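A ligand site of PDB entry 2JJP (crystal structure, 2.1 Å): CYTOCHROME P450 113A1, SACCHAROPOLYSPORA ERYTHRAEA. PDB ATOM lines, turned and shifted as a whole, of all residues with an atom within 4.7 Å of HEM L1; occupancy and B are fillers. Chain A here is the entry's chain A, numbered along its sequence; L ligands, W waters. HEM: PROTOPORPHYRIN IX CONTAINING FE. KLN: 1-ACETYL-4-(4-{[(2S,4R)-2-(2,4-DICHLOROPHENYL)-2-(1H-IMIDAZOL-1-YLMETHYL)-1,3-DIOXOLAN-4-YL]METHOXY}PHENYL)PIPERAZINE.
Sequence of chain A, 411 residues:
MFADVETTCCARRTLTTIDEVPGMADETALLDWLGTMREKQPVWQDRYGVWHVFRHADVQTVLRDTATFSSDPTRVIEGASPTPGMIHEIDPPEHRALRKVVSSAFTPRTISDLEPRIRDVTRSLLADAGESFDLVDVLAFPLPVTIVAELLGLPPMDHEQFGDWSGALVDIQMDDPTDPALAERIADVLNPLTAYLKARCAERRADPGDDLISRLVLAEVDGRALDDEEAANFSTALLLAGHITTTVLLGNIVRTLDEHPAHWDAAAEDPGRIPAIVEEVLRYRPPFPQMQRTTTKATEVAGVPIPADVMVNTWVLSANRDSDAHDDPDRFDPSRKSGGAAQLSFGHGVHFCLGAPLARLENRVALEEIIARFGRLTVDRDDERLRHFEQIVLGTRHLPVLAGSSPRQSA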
ATOM      1  N   ILE A  87       7.430   2.390  20.154  1.00  0.00           N
ATOM      2  CA  ILE A  87       6.021   2.625  19.902  1.00  0.00           C
ATOM      3  C   ILE A  87       5.709   3.673  18.797  1.00  0.00           C
ATOM      4  O   ILE A  87       4.656   3.633  18.158  1.00  0.00           O
ATOM      5  CB  ILE A  87       5.327   2.898  21.268  1.00  0.00           C
ATOM      6  CG1 ILE A  87       3.813   2.789  21.177  1.00  0.00           C
ATOM      7  CG2 ILE A  87       5.832   4.209  21.903  1.00  0.00           C
ATOM      8  CD1 ILE A  87       3.121   3.037  22.514  1.00  0.00           C
ATOM      9  N   HIS A  88       6.646   4.579  18.556  1.00  0.00           N
ATOM     10  CA  HIS A  88       6.512   5.609  17.543  1.00  0.00           C
ATOM     11  C   HIS A  88       6.926   5.135  16.135  1.00  0.00           C
ATOM     12  O   HIS A  88       6.851   5.862  15.153  1.00  0.00           O
ATOM     13  CB  HIS A  88       7.316   6.836  17.949  1.00  0.00           C
ATOM     14  CG  HIS A  88       8.796   6.699  17.742  1.00  0.00           C
ATOM     15  ND1 HIS A  88       9.601   5.919  18.553  1.00  0.00           N
ATOM     16  CD2 HIS A  88       9.621   7.290  16.847  1.00  0.00           C
ATOM     17  CE1 HIS A  88      10.855   6.030  18.148  1.00  0.00           C
ATOM     18  NE2 HIS A  88      10.893   6.855  17.121  1.00  0.00           N
ATOM     19  N   HIS A  95       0.624  -1.370  17.285  1.00  0.00           N
ATOM     20  CA  HIS A  95       0.673  -0.079  17.998  1.00  0.00           C
ATOM     21  C   HIS A  95      -0.416   0.031  19.060  1.00  0.00           C
ATOM     22  O   HIS A  95      -0.162   0.487  20.160  1.00  0.00           O
ATOM     23  CB  HIS A  95       0.493   1.107  17.054  1.00  0.00           C
ATOM     24  CG  HIS A  95       0.454   2.416  17.781  1.00  0.00           C
ATOM     25  ND1 HIS A  95      -0.727   3.114  18.008  1.00  0.00           N
ATOM     26  CD2 HIS A  95       1.429   3.124  18.383  1.00  0.00           C
ATOM     27  CE1 HIS A  95      -0.449   4.222  18.673  1.00  0.00           C
ATOM     28  NE2 HIS A  95       0.842   4.249  18.931  1.00  0.00           N
ATOM     29  N   ARG A  99       0.502   0.479  22.851  1.00  0.00           N
ATOM     30  CA  ARG A  99       0.107   1.710  23.512  1.00  0.00           C
ATOM     31  C   ARG A  99      -0.699   1.425  24.761  1.00  0.00           C
ATOM     32  O   ARG A  99      -0.480   2.056  25.803  1.00  0.00           O
ATOM     33  CB  ARG A  99      -0.685   2.624  22.588  1.00  0.00           C
ATOM     34  CG  ARG A  99      -1.194   3.886  23.276  1.00  0.00           C
ATOM     35  CD  ARG A  99      -0.416   5.061  22.801  1.00  0.00           C
ATOM     36  NE  ARG A  99      -0.821   6.302  23.453  1.00  0.00           N
ATOM     37  CZ  ARG A  99      -0.518   7.517  22.979  1.00  0.00           C
ATOM     38  NH1 ARG A  99       0.160   7.606  21.853  1.00  0.00           N
ATOM     39  NH2 ARG A  99      -0.895   8.633  23.623  1.00  0.00           N
ATOM     40  N   PHE A 106       2.198   4.066  32.670  1.00  0.00           N
ATOM     41  CA  PHE A 106       2.501   5.499  32.556  1.00  0.00           C
ATOM     42  C   PHE A 106       1.228   6.333  32.708  1.00  0.00           C
ATOM     43  O   PHE A 106       0.628   6.771  31.732  1.00  0.00           O
ATOM     44  CB  PHE A 106       3.185   5.765  31.199  1.00  0.00           C
ATOM     45  CG  PHE A 106       3.900   7.083  31.106  1.00  0.00           C
ATOM     46  CD1 PHE A 106       5.172   7.228  31.658  1.00  0.00           C
ATOM     47  CD2 PHE A 106       3.341   8.162  30.433  1.00  0.00           C
ATOM     48  CE1 PHE A 106       5.865   8.434  31.554  1.00  0.00           C
ATOM     49  CE2 PHE A 106       4.014   9.370  30.332  1.00  0.00           C
ATOM     50  CZ  PHE A 106       5.295   9.504  30.885  1.00  0.00           C
ATOM     51  N   PHE A 234      11.576   0.765  25.006  1.00  0.00           N
ATOM     52  CA  PHE A 234      10.651   1.838  25.338  1.00  0.00           C
ATOM     53  C   PHE A 234      11.164   2.728  26.472  1.00  0.00           C
ATOM     54  O   PHE A 234      10.979   3.928  26.421  1.00  0.00           O
ATOM     55  CB  PHE A 234       9.254   1.290  25.676  1.00  0.00           C
ATOM     56  CG  PHE A 234       8.254   2.373  26.041  1.00  0.00           C
ATOM     57  CD1 PHE A 234       7.709   3.191  25.063  1.00  0.00           C
ATOM     58  CD2 PHE A 234       7.859   2.549  27.364  1.00  0.00           C
ATOM     59  CE1 PHE A 234       6.766   4.203  25.385  1.00  0.00           C
ATOM     60  CE2 PHE A 234       6.931   3.544  27.716  1.00  0.00           C
ATOM     61  CZ  PHE A 234       6.393   4.379  26.714  1.00  0.00           C
ATOM     62  N   LEU A 238      11.860   6.922  26.349  1.00  0.00           N
ATOM     63  CA  LEU A 238      11.485   7.807  27.476  1.00  0.00           C
ATOM     64  C   LEU A 238      12.655   8.636  28.024  1.00  0.00           C
ATOM     65  O   LEU A 238      12.486   9.834  28.298  1.00  0.00           O
ATOM     66  CB  LEU A 238      10.915   6.973  28.614  1.00  0.00           C
ATOM     67  CG  LEU A 238       9.397   6.818  28.756  1.00  0.00           C
ATOM     68  CD1 LEU A 238       8.548   7.178  27.499  1.00  0.00           C
ATOM     69  CD2 LEU A 238       9.111   5.448  29.290  1.00  0.00           C
ATOM     70  N   ALA A 241      13.573  11.180  25.420  1.00  0.00           N
ATOM     71  CA  ALA A 241      12.560  12.257  25.541  1.00  0.00           C
ATOM     72  C   ALA A 241      12.923  13.204  26.655  1.00  0.00           C
ATOM     73  O   ALA A 241      12.911  14.424  26.475  1.00  0.00           O
ATOM     74  CB  ALA A 241      11.151  11.654  25.777  1.00  0.00           C
ATOM     75  N   THR A 245      13.454  17.128  25.090  1.00  0.00           N
ATOM     76  CA  THR A 245      12.190  17.857  24.886  1.00  0.00           C
ATOM     77  C   THR A 245      11.995  19.105  25.744  1.00  0.00           C
ATOM     78  O   THR A 245      11.858  20.198  25.205  1.00  0.00           O
ATOM     79  CB  THR A 245      11.002  16.913  25.108  1.00  0.00           C
ATOM     80  OG1 THR A 245      11.143  16.320  26.397  1.00  0.00           O
ATOM     81  CG2 THR A 245      11.030  15.833  24.083  1.00  0.00           C
ATOM     82  N   THR A 246      11.978  18.962  27.061  1.00  0.00           N
ATOM     83  CA  THR A 246      11.950  20.110  27.994  1.00  0.00           C
ATOM     84  C   THR A 246      13.190  20.976  27.815  1.00  0.00           C
ATOM     85  O   THR A 246      13.114  22.174  27.928  1.00  0.00           O
ATOM     86  CB  THR A 246      11.799  19.682  29.510  1.00  0.00           C
ATOM     87  OG1 THR A 246      10.432  19.346  29.793  1.00  0.00           O
ATOM     88  CG2 THR A 246      12.200  20.814  30.457  1.00  0.00           C
ATOM     89  N   LEU A 249      12.076  22.986  24.773  1.00  0.00           N
ATOM     90  CA  LEU A 249      10.882  23.823  24.972  1.00  0.00           C
ATOM     91  C   LEU A 249      11.172  24.962  25.919  1.00  0.00           C
ATOM     92  O   LEU A 249      10.768  26.073  25.654  1.00  0.00           O
ATOM     93  CB  LEU A 249       9.697  23.006  25.494  1.00  0.00           C
ATOM     94  CG  LEU A 249       8.380  23.774  25.726  1.00  0.00           C
ATOM     95  CD1 LEU A 249       7.849  24.637  24.513  1.00  0.00           C
ATOM     96  CD2 LEU A 249       7.236  22.844  26.255  1.00  0.00           C
ATOM     97  N   LEU A 282       4.506  26.473  22.448  1.00  0.00           N
ATOM     98  CA  LEU A 282       4.376  25.178  21.740  1.00  0.00           C
ATOM     99  C   LEU A 282       3.904  25.314  20.310  1.00  0.00           C
ATOM    100  O   LEU A 282       4.474  24.703  19.395  1.00  0.00           O
ATOM    101  CB  LEU A 282       3.443  24.237  22.489  1.00  0.00           C
ATOM    102  CG  LEU A 282       4.123  23.365  23.510  1.00  0.00           C
ATOM    103  CD1 LEU A 282       3.047  22.617  24.331  1.00  0.00           C
ATOM    104  CD2 LEU A 282       5.129  22.368  22.845  1.00  0.00           C
ATOM    105  N   PRO A 287       9.192  22.388  19.431  1.00  0.00           N
ATOM    106  CA  PRO A 287      10.484  21.739  19.577  1.00  0.00           C
ATOM    107  C   PRO A 287      10.778  20.842  18.405  1.00  0.00           C
ATOM    108  O   PRO A 287      11.926  20.846  17.912  1.00  0.00           O
ATOM    109  CB  PRO A 287      10.321  20.933  20.871  1.00  0.00           C
ATOM    110  CG  PRO A 287       9.422  21.805  21.688  1.00  0.00           C
ATOM    111  CD  PRO A 287       8.398  22.272  20.664  1.00  0.00           C
ATOM    112  N   PHE A 288       9.759  20.102  17.971  1.00  0.00           N
ATOM    113  CA  PHE A 288       9.832  19.267  16.781  1.00  0.00           C
ATOM    114  C   PHE A 288       9.032  19.798  15.603  1.00  0.00           C
ATOM    115  O   PHE A 288       7.813  19.559  15.516  1.00  0.00           O
ATOM    116  CB  PHE A 288       9.440  17.820  17.098  1.00  0.00           C
ATOM    117  CG  PHE A 288      10.312  17.177  18.165  1.00  0.00           C
ATOM    118  CD1 PHE A 288       9.787  16.908  19.441  1.00  0.00           C
ATOM    119  CD2 PHE A 288      11.613  16.861  17.904  1.00  0.00           C
ATOM    120  CE1 PHE A 288      10.565  16.344  20.453  1.00  0.00           C
ATOM    121  CE2 PHE A 288      12.425  16.270  18.892  1.00  0.00           C
ATOM    122  CZ  PHE A 288      11.894  16.023  20.177  1.00  0.00           C
ATOM    123  N   MET A 291       7.597  15.942  11.442  1.00  0.00           N
ATOM    124  CA  MET A 291       7.412  14.504  11.709  1.00  0.00           C
ATOM    125  C   MET A 291       7.503  13.772  10.398  1.00  0.00           C
ATOM    126  O   MET A 291       7.387  14.381   9.359  1.00  0.00           O
ATOM    127  CB  MET A 291       6.045  14.246  12.362  1.00  0.00           C
ATOM    128  CG  MET A 291       5.921  14.772  13.769  1.00  0.00           C
ATOM    129  SD  MET A 291       4.361  15.613  13.975  1.00  0.00           S
ATOM    130  CE  MET A 291       4.903  16.870  15.135  1.00  0.00           C
ATOM    131  N   ARG A 293       6.745  10.210   7.856  1.00  0.00           N
ATOM    132  CA  ARG A 293       5.928   9.027   7.529  1.00  0.00           C
ATOM    133  C   ARG A 293       6.441   8.411   6.235  1.00  0.00           C
ATOM    134  O   ARG A 293       7.214   9.038   5.550  1.00  0.00           O
ATOM    135  CB  ARG A 293       4.447   9.392   7.375  1.00  0.00           C
ATOM    136  CG  ARG A 293       3.806  10.086   8.600  1.00  0.00           C
ATOM    137  CD  ARG A 293       3.601   9.062   9.706  1.00  0.00           C
ATOM    138  NE  ARG A 293       2.823   9.472  10.873  1.00  0.00           N
ATOM    139  CZ  ARG A 293       3.376   9.997  11.959  1.00  0.00           C
ATOM    140  NH1 ARG A 293       4.699  10.214  12.009  1.00  0.00           N
ATOM    141  NH2 ARG A 293       2.650  10.305  13.007  1.00  0.00           N
ATOM    142  N   SER A 345       1.591  20.401  18.085  1.00  0.00           N
ATOM    143  CA  SER A 345       3.014  20.206  18.338  1.00  0.00           C
ATOM    144  C   SER A 345       3.295  18.934  19.091  1.00  0.00           C
ATOM    145  O   SER A 345       4.472  18.551  19.201  1.00  0.00           O
ATOM    146  CB  SER A 345       3.629  21.413  19.070  1.00  0.00           C
ATOM    147  OG  SER A 345       3.474  22.589  18.277  1.00  0.00           O
ATOM    148  N   PHE A 346       2.260  18.301  19.620  1.00  0.00           N
ATOM    149  CA  PHE A 346       2.417  17.019  20.253  1.00  0.00           C
ATOM    150  C   PHE A 346       1.959  15.922  19.312  1.00  0.00           C
ATOM    151  O   PHE A 346       1.750  14.787  19.757  1.00  0.00           O
ATOM    152  CB  PHE A 346       1.594  16.923  21.541  1.00  0.00           C
ATOM    153  CG  PHE A 346       2.155  17.658  22.739  1.00  0.00           C
ATOM    154  CD1 PHE A 346       1.348  18.564  23.421  1.00  0.00           C
ATOM    155  CD2 PHE A 346       3.380  17.363  23.249  1.00  0.00           C
ATOM    156  CE1 PHE A 346       1.828  19.249  24.529  1.00  0.00           C
ATOM    157  CE2 PHE A 346       3.891  18.047  24.362  1.00  0.00           C
ATOM    158  CZ  PHE A 346       3.101  18.978  25.016  1.00  0.00           C
ATOM    159  N   GLY A 347       1.679  16.275  18.052  1.00  0.00           N
ATOM    160  CA  GLY A 347       1.364  15.293  16.995  1.00  0.00           C
ATOM    161  C   GLY A 347      -0.171  15.251  16.806  1.00  0.00           C
ATOM    162  O   GLY A 347      -0.873  16.158  17.273  1.00  0.00           O
ATOM    163  N   VAL A 350      -3.241   8.611  16.568  1.00  0.00           N
ATOM    164  CA  VAL A 350      -2.929   7.585  17.547  1.00  0.00           C
ATOM    165  C   VAL A 350      -1.509   7.651  18.114  1.00  0.00           C
ATOM    166  O   VAL A 350      -1.221   7.030  19.153  1.00  0.00           O
ATOM    167  CB  VAL A 350      -3.198   6.176  16.973  1.00  0.00           C
ATOM    168  CG1 VAL A 350      -4.695   6.013  16.599  1.00  0.00           C
ATOM    169  CG2 VAL A 350      -2.276   5.881  15.753  1.00  0.00           C
ATOM    170  N   HIS A 351      -0.613   8.373  17.444  1.00  0.00           N
ATOM    171  CA  HIS A 351       0.718   8.512  17.986  1.00  0.00           C
ATOM    172  C   HIS A 351       0.863   9.771  18.861  1.00  0.00           C
ATOM    173  O   HIS A 351       1.956  10.128  19.273  1.00  0.00           O
ATOM    174  CB  HIS A 351       1.768   8.436  16.865  1.00  0.00           C
ATOM    175  CG  HIS A 351       1.926   7.058  16.269  1.00  0.00           C
ATOM    176  ND1 HIS A 351       2.674   6.066  16.863  1.00  0.00           N
ATOM    177  CD2 HIS A 351       1.394   6.505  15.142  1.00  0.00           C
ATOM    178  CE1 HIS A 351       2.647   4.980  16.107  1.00  0.00           C
ATOM    179  NE2 HIS A 351       1.873   5.214  15.058  1.00  0.00           N
ATOM    180  N   PHE A 352      -0.268  10.455  19.151  1.00  0.00           N
ATOM    181  CA  PHE A 352      -0.250  11.673  19.963  1.00  0.00           C
ATOM    182  C   PHE A 352       0.617  11.505  21.221  1.00  0.00           C
ATOM    183  O   PHE A 352       0.505  10.520  21.965  1.00  0.00           O
ATOM    184  CB  PHE A 352      -1.661  12.050  20.380  1.00  0.00           C
ATOM    185  CG  PHE A 352      -1.787  13.446  20.978  1.00  0.00           C
ATOM    186  CD1 PHE A 352      -2.114  14.522  20.180  1.00  0.00           C
ATOM    187  CD2 PHE A 352      -1.539  13.668  22.338  1.00  0.00           C
ATOM    188  CE1 PHE A 352      -2.204  15.782  20.698  1.00  0.00           C
ATOM    189  CE2 PHE A 352      -1.650  14.966  22.896  1.00  0.00           C
ATOM    190  CZ  PHE A 352      -1.956  16.014  22.057  1.00  0.00           C
ATOM    191  N   CYS A 353       1.447  12.514  21.478  1.00  0.00           N
ATOM    192  CA  CYS A 353       2.426  12.473  22.553  1.00  0.00           C
ATOM    193  C   CYS A 353       1.959  11.882  23.864  1.00  0.00           C
ATOM    194  O   CYS A 353       1.068  12.437  24.538  1.00  0.00           O
ATOM    195  CB  CYS A 353       3.038  13.837  22.781  1.00  0.00           C
ATOM    196  SG  CYS A 353       4.495  13.739  23.816  1.00  0.00           S
ATOM    197  N   LEU A 354       2.590  10.785  24.249  1.00  0.00           N
ATOM    198  CA  LEU A 354       2.245  10.086  25.500  1.00  0.00           C
ATOM    199  C   LEU A 354       2.753  10.848  26.725  1.00  0.00           C
ATOM    200  O   LEU A 354       2.166  10.790  27.830  1.00  0.00           O
ATOM    201  CB  LEU A 354       2.764   8.632  25.494  1.00  0.00           C
ATOM    202  CG  LEU A 354       2.427   7.744  26.708  1.00  0.00           C
ATOM    203  CD1 LEU A 354       0.922   7.462  26.815  1.00  0.00           C
ATOM    204  CD2 LEU A 354       3.212   6.407  26.646  1.00  0.00           C
ATOM    205  N   GLY A 355       3.816  11.600  26.523  1.00  0.00           N
ATOM    206  CA  GLY A 355       4.459  12.323  27.616  1.00  0.00           C
ATOM    207  C   GLY A 355       3.960  13.763  27.743  1.00  0.00           C
ATOM    208  O   GLY A 355       4.472  14.518  28.589  1.00  0.00           O
ATOM    209  N   LEU A 358       3.472  15.230  31.244  1.00  0.00           N
ATOM    210  CA  LEU A 358       4.734  15.411  31.897  1.00  0.00           C
ATOM    211  C   LEU A 358       5.419  16.656  31.378  1.00  0.00           C
ATOM    212  O   LEU A 358       5.897  17.457  32.182  1.00  0.00           O
ATOM    213  CB  LEU A 358       5.614  14.147  31.755  1.00  0.00           C
ATOM    214  CG  LEU A 358       7.059  14.169  32.313  1.00  0.00           C
ATOM    215  CD1 LEU A 358       7.095  14.730  33.747  1.00  0.00           C
ATOM    216  CD2 LEU A 358       7.617  12.787  32.320  1.00  0.00           C
ATOM    217  N   ALA A 359       5.463  16.859  30.067  1.00  0.00           N
ATOM    218  CA  ALA A 359       6.152  18.071  29.532  1.00  0.00           C
ATOM    219  C   ALA A 359       5.461  19.368  30.034  1.00  0.00           C
ATOM    220  O   ALA A 359       6.111  20.323  30.456  1.00  0.00           O
ATOM    221  CB  ALA A 359       6.182  18.033  28.032  1.00  0.00           C
HETATM  222  CHA HEM L   1       5.083  11.238  20.554  1.00  0.00           C
HETATM  223  CHB HEM L   1       6.226  15.907  20.814  1.00  0.00           C
HETATM  224  CHC HEM L   1       7.660  15.449  25.468  1.00  0.00           C
HETATM  225  CHD HEM L   1       7.121  10.668  24.925  1.00  0.00           C
HETATM  226  C1A HEM L   1       5.240  12.558  20.237  1.00  0.00           C
HETATM  227  C2A HEM L   1       4.895  13.135  18.957  1.00  0.00           C
HETATM  228  C3A HEM L   1       5.211  14.444  19.033  1.00  0.00           C
HETATM  229  C4A HEM L   1       5.790  14.698  20.347  1.00  0.00           C
HETATM  230  CMA HEM L   1       5.081  15.525  17.960  1.00  0.00           C
HETATM  231  CAA HEM L   1       4.259  12.318  17.784  1.00  0.00           C
HETATM  232  CBA HEM L   1       5.391  11.683  16.952  1.00  0.00           C
HETATM  233  CGA HEM L   1       4.806  11.107  15.653  1.00  0.00           C
HETATM  234  O1A HEM L   1       3.594  11.203  15.374  1.00  0.00           O
HETATM  235  O2A HEM L   1       5.582  10.549  14.847  1.00  0.00           O
HETATM  236  C1B HEM L   1       6.669  16.176  22.101  1.00  0.00           C
HETATM  237  C2B HEM L   1       7.033  17.462  22.581  1.00  0.00           C
HETATM  238  C3B HEM L   1       7.450  17.347  23.864  1.00  0.00           C
HETATM  239  C4B HEM L   1       7.350  15.972  24.240  1.00  0.00           C
HETATM  240  CMB HEM L   1       6.877  18.704  21.686  1.00  0.00           C
HETATM  241  CAB HEM L   1       7.908  18.434  24.869  1.00  0.00           C
HETATM  242  CBB HEM L   1       8.038  19.686  24.494  1.00  0.00           C
HETATM  243  C1C HEM L   1       7.666  14.092  25.739  1.00  0.00           C
HETATM  244  C2C HEM L   1       8.085  13.431  26.965  1.00  0.00           C
HETATM  245  C3C HEM L   1       7.903  12.117  26.783  1.00  0.00           C
HETATM  246  C4C HEM L   1       7.377  11.918  25.451  1.00  0.00           C
HETATM  247  CMC HEM L   1       8.607  14.120  28.250  1.00  0.00           C
HETATM  248  CAC HEM L   1       8.161  10.942  27.762  1.00  0.00           C
HETATM  249  CBC HEM L   1       8.869  11.050  28.898  1.00  0.00           C
HETATM  250  C1D HEM L   1       6.478  10.357  23.744  1.00  0.00           C
HETATM  251  C2D HEM L   1       6.036   9.039  23.354  1.00  0.00           C
HETATM  252  C3D HEM L   1       5.372   9.216  21.975  1.00  0.00           C
HETATM  253  C4D HEM L   1       5.558  10.607  21.673  1.00  0.00           C
HETATM  254  CMD HEM L   1       6.255   7.768  24.221  1.00  0.00           C
HETATM  255  CAD HEM L   1       4.758   8.200  20.969  1.00  0.00           C
HETATM  256  CBD HEM L   1       3.427   7.606  21.364  1.00  0.00           C
HETATM  257  CGD HEM L   1       2.937   6.621  20.351  1.00  0.00           C
HETATM  258  O1D HEM L   1       3.666   6.324  19.373  1.00  0.00           O
HETATM  259  O2D HEM L   1       1.789   6.149  20.561  1.00  0.00           O
HETATM  260  NA  HEM L   1       5.767  13.521  21.061  1.00  0.00           N
HETATM  261  NB  HEM L   1       6.843  15.272  23.160  1.00  0.00           N
HETATM  262  NC  HEM L   1       7.246  13.148  24.821  1.00  0.00           N
HETATM  263  ND  HEM L   1       6.188  11.245  22.729  1.00  0.00           N
HETATM  264 FE   HEM L   1       6.487  13.262  22.924  1.00  0.00          FE
HETATM  265  N1  KLN L   2       9.995  12.903  20.847  1.00  0.00           N
HETATM  266  C1  KLN L   2       8.749  13.390  20.992  1.00  0.00           C
HETATM  267  N2  KLN L   2       8.325  13.142  22.247  1.00  0.00           N
HETATM  268  C2  KLN L   2       9.303  12.477  22.885  1.00  0.00           C
HETATM  269  C3  KLN L   2      10.358  12.335  21.999  1.00  0.00           C
HETATM  270  C4  KLN L   2      10.782  12.938  19.616  1.00  0.00           C
HETATM  271  C5  KLN L   2      10.252  11.788  18.758  1.00  0.00           C
HETATM  272  O1  KLN L   2      11.129  11.497  17.689  1.00  0.00           O
HETATM  273  C6  KLN L   2      10.327  10.964  16.641  1.00  0.00           C
HETATM  274  C7  KLN L   2       8.942  11.525  16.883  1.00  0.00           C
HETATM  275  O2  KLN L   2       9.019  12.142  18.169  1.00  0.00           O
HETATM  276  C8  KLN L   2       9.985  10.522  19.520  1.00  0.00           C
HETATM  277  C9  KLN L   2      11.017   9.766  20.048  1.00  0.00           C
HETATM  278  C10 KLN L   2      10.730   8.605  20.758  1.00  0.00           C
HETATM  279  C11 KLN L   2       9.397   8.227  20.907  1.00  0.00           C
HETATM  280  C12 KLN L   2       8.375   8.992  20.375  1.00  0.00           C
HETATM  281  C13 KLN L   2       8.663  10.144  19.677  1.00  0.00           C
HETATM  282 CL1  KLN L   2       8.948   6.758  21.783  1.00  0.00          CL
HETATM  283  C14 KLN L   2      10.790  11.414  15.269  1.00  0.00           C
HETATM  284  O3  KLN L   2      11.255  12.760  15.188  1.00  0.00           O
HETATM  285  C15 KLN L   2      11.852  13.089  14.002  1.00  0.00           C
HETATM  286  C16 KLN L   2      11.259  14.012  13.162  1.00  0.00           C
HETATM  287  C17 KLN L   2      11.861  14.336  11.946  1.00  0.00           C
HETATM  288  C18 KLN L   2      13.063  13.752  11.546  1.00  0.00           C
HETATM  289  C19 KLN L   2      13.654  12.798  12.391  1.00  0.00           C
HETATM  290  C20 KLN L   2      13.054  12.476  13.616  1.00  0.00           C
HETATM  291  N3  KLN L   2      13.637  14.090  10.282  1.00  0.00           N
HETATM  292  C21 KLN L   2      13.212  15.427   9.835  1.00  0.00           C
HETATM  293  C22 KLN L   2      14.334  16.167   9.110  1.00  0.00           C
HETATM  294  N4  KLN L   2      15.083  15.299   8.187  1.00  0.00           N
HETATM  295  C23 KLN L   2      15.605  14.077   8.836  1.00  0.00           C
HETATM  296  C24 KLN L   2      15.112  13.973  10.268  1.00  0.00           C
HETATM  297  C25 KLN L   2      16.161  16.035   7.615  1.00  0.00           C
HETATM  298  O4  KLN L   2      16.998  16.596   8.324  1.00  0.00           O
HETATM  299  C26 KLN L   2      16.275  16.125   6.122  1.00  0.00           C
HETATM  300 CL2  KLN L   2      12.697  10.293  19.823  1.00  0.00          CL
HETATM  301  O   HOH W   1       4.866   7.705  14.907  1.00  0.00           O
HETATM  302  O   HOH W   2       7.789   8.469  14.499  1.00  0.00           O
HETATM  303  O   HOH W   3       8.077  11.768  13.324  1.00  0.00           O
HETATM  304  O   HOH W   4       1.134  12.165  15.731  1.00  0.00           O
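Water W1 lies within hydrogen-bond range of O of His 88 (2.7 Å), O2A of HEM L1 (2.9 Å) and ND1 of His 351 (3.4 Å). Water W2 lies within hydrogen-bond range of the backbone carbonyl oxygen of His 88 and an oxygen (O2A) of HEM L1.
An oxygen (O1D) of HEM L1 lies close to the backbone carbonyl oxygen (O) of Ile 87. An oxygen (O2D) of HEM L1 sits close to the backbone carbonyl oxygen (O) of Val 350, at 3.4 Å. Merely in contact with HEM L1: Met 291 (3.1 Å), Ser 345 (3.3 Å), Phe 346 (3.4 Å), Ala 241 (3.4 Å), Thr 245 (3.5 Å), His 88 (3.5 Å), Gly 347 (3.5 Å), Gly 355 (3.5 Å), Ala 359 (3.6 Å), Leu 249 (3.7 Å), Pro 287 (3.8 Å), Phe 234 (3.8 Å), Leu 238 (3.8 Å), Leu 354 (3.8 Å) and Phe 288 (3.9 Å). Hydrophobic or aromatic side chains within 4 Å of HEM L1: Ile 87, His 88, His 95, Phe 234, Leu 238, Ala 241, Leu 249, Pro 287, Phe 288, Met 291, Phe 346, His 351, Leu 354 and Ala 359. Along chain A the residues within 4 Å of HEM L1 span positions 87 to 359.
A nitrogen (N2) of KLN L2 binds an iron atom (FE) of HEM L1, at 2.0 Å.
O2D of HEM L1 lies within salt-bridge range of NH1 of Arg 99 (2.5 Å). An oxygen (O1A) of HEM L1 is in salt-bridge range of the guanidinium group (NH2) of Arg 293. A ring nitrogen (NE2) of His 95 is in hydrogen-bond range of an oxygen (O2D) of HEM L1, 2.7 Å away. ND1 of His 351 is in hydrogen-bond range of O1D of HEM L1 (2.7 Å). SG of Cys 353 is bound to FE of HEM L1, 2.2 Å away.
OG of Ser 345 lies within hydrogen-bond range of O of Leu 282, 2.6 Å away. The backbone NH of Cys 353 lies within hydrogen-bond range of the backbone carbonyl oxygen of Phe 346 (2.9 Å). ND1 of His 351 lies within hydrogen-bond range of NE2 of His 95 (3.3 Å). The side-chain sulfur (SG) of Cys 353 lies close to the backbone NH (N) of Gly 355 (3.5 Å). ND1 of His 351 sits close to O of Ile 87 (3.4 Å). NE2 of His 95 sits close to O of Val 350 (3.5 Å). O of Phe 352 sits at hydrogen-bond distance from NH2 of Arg 99. The side-chain hydroxyl (OG1) of Thr 245 sits at hydrogen-bond distance from the backbone carbonyl oxygen (O) of Ala 241.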
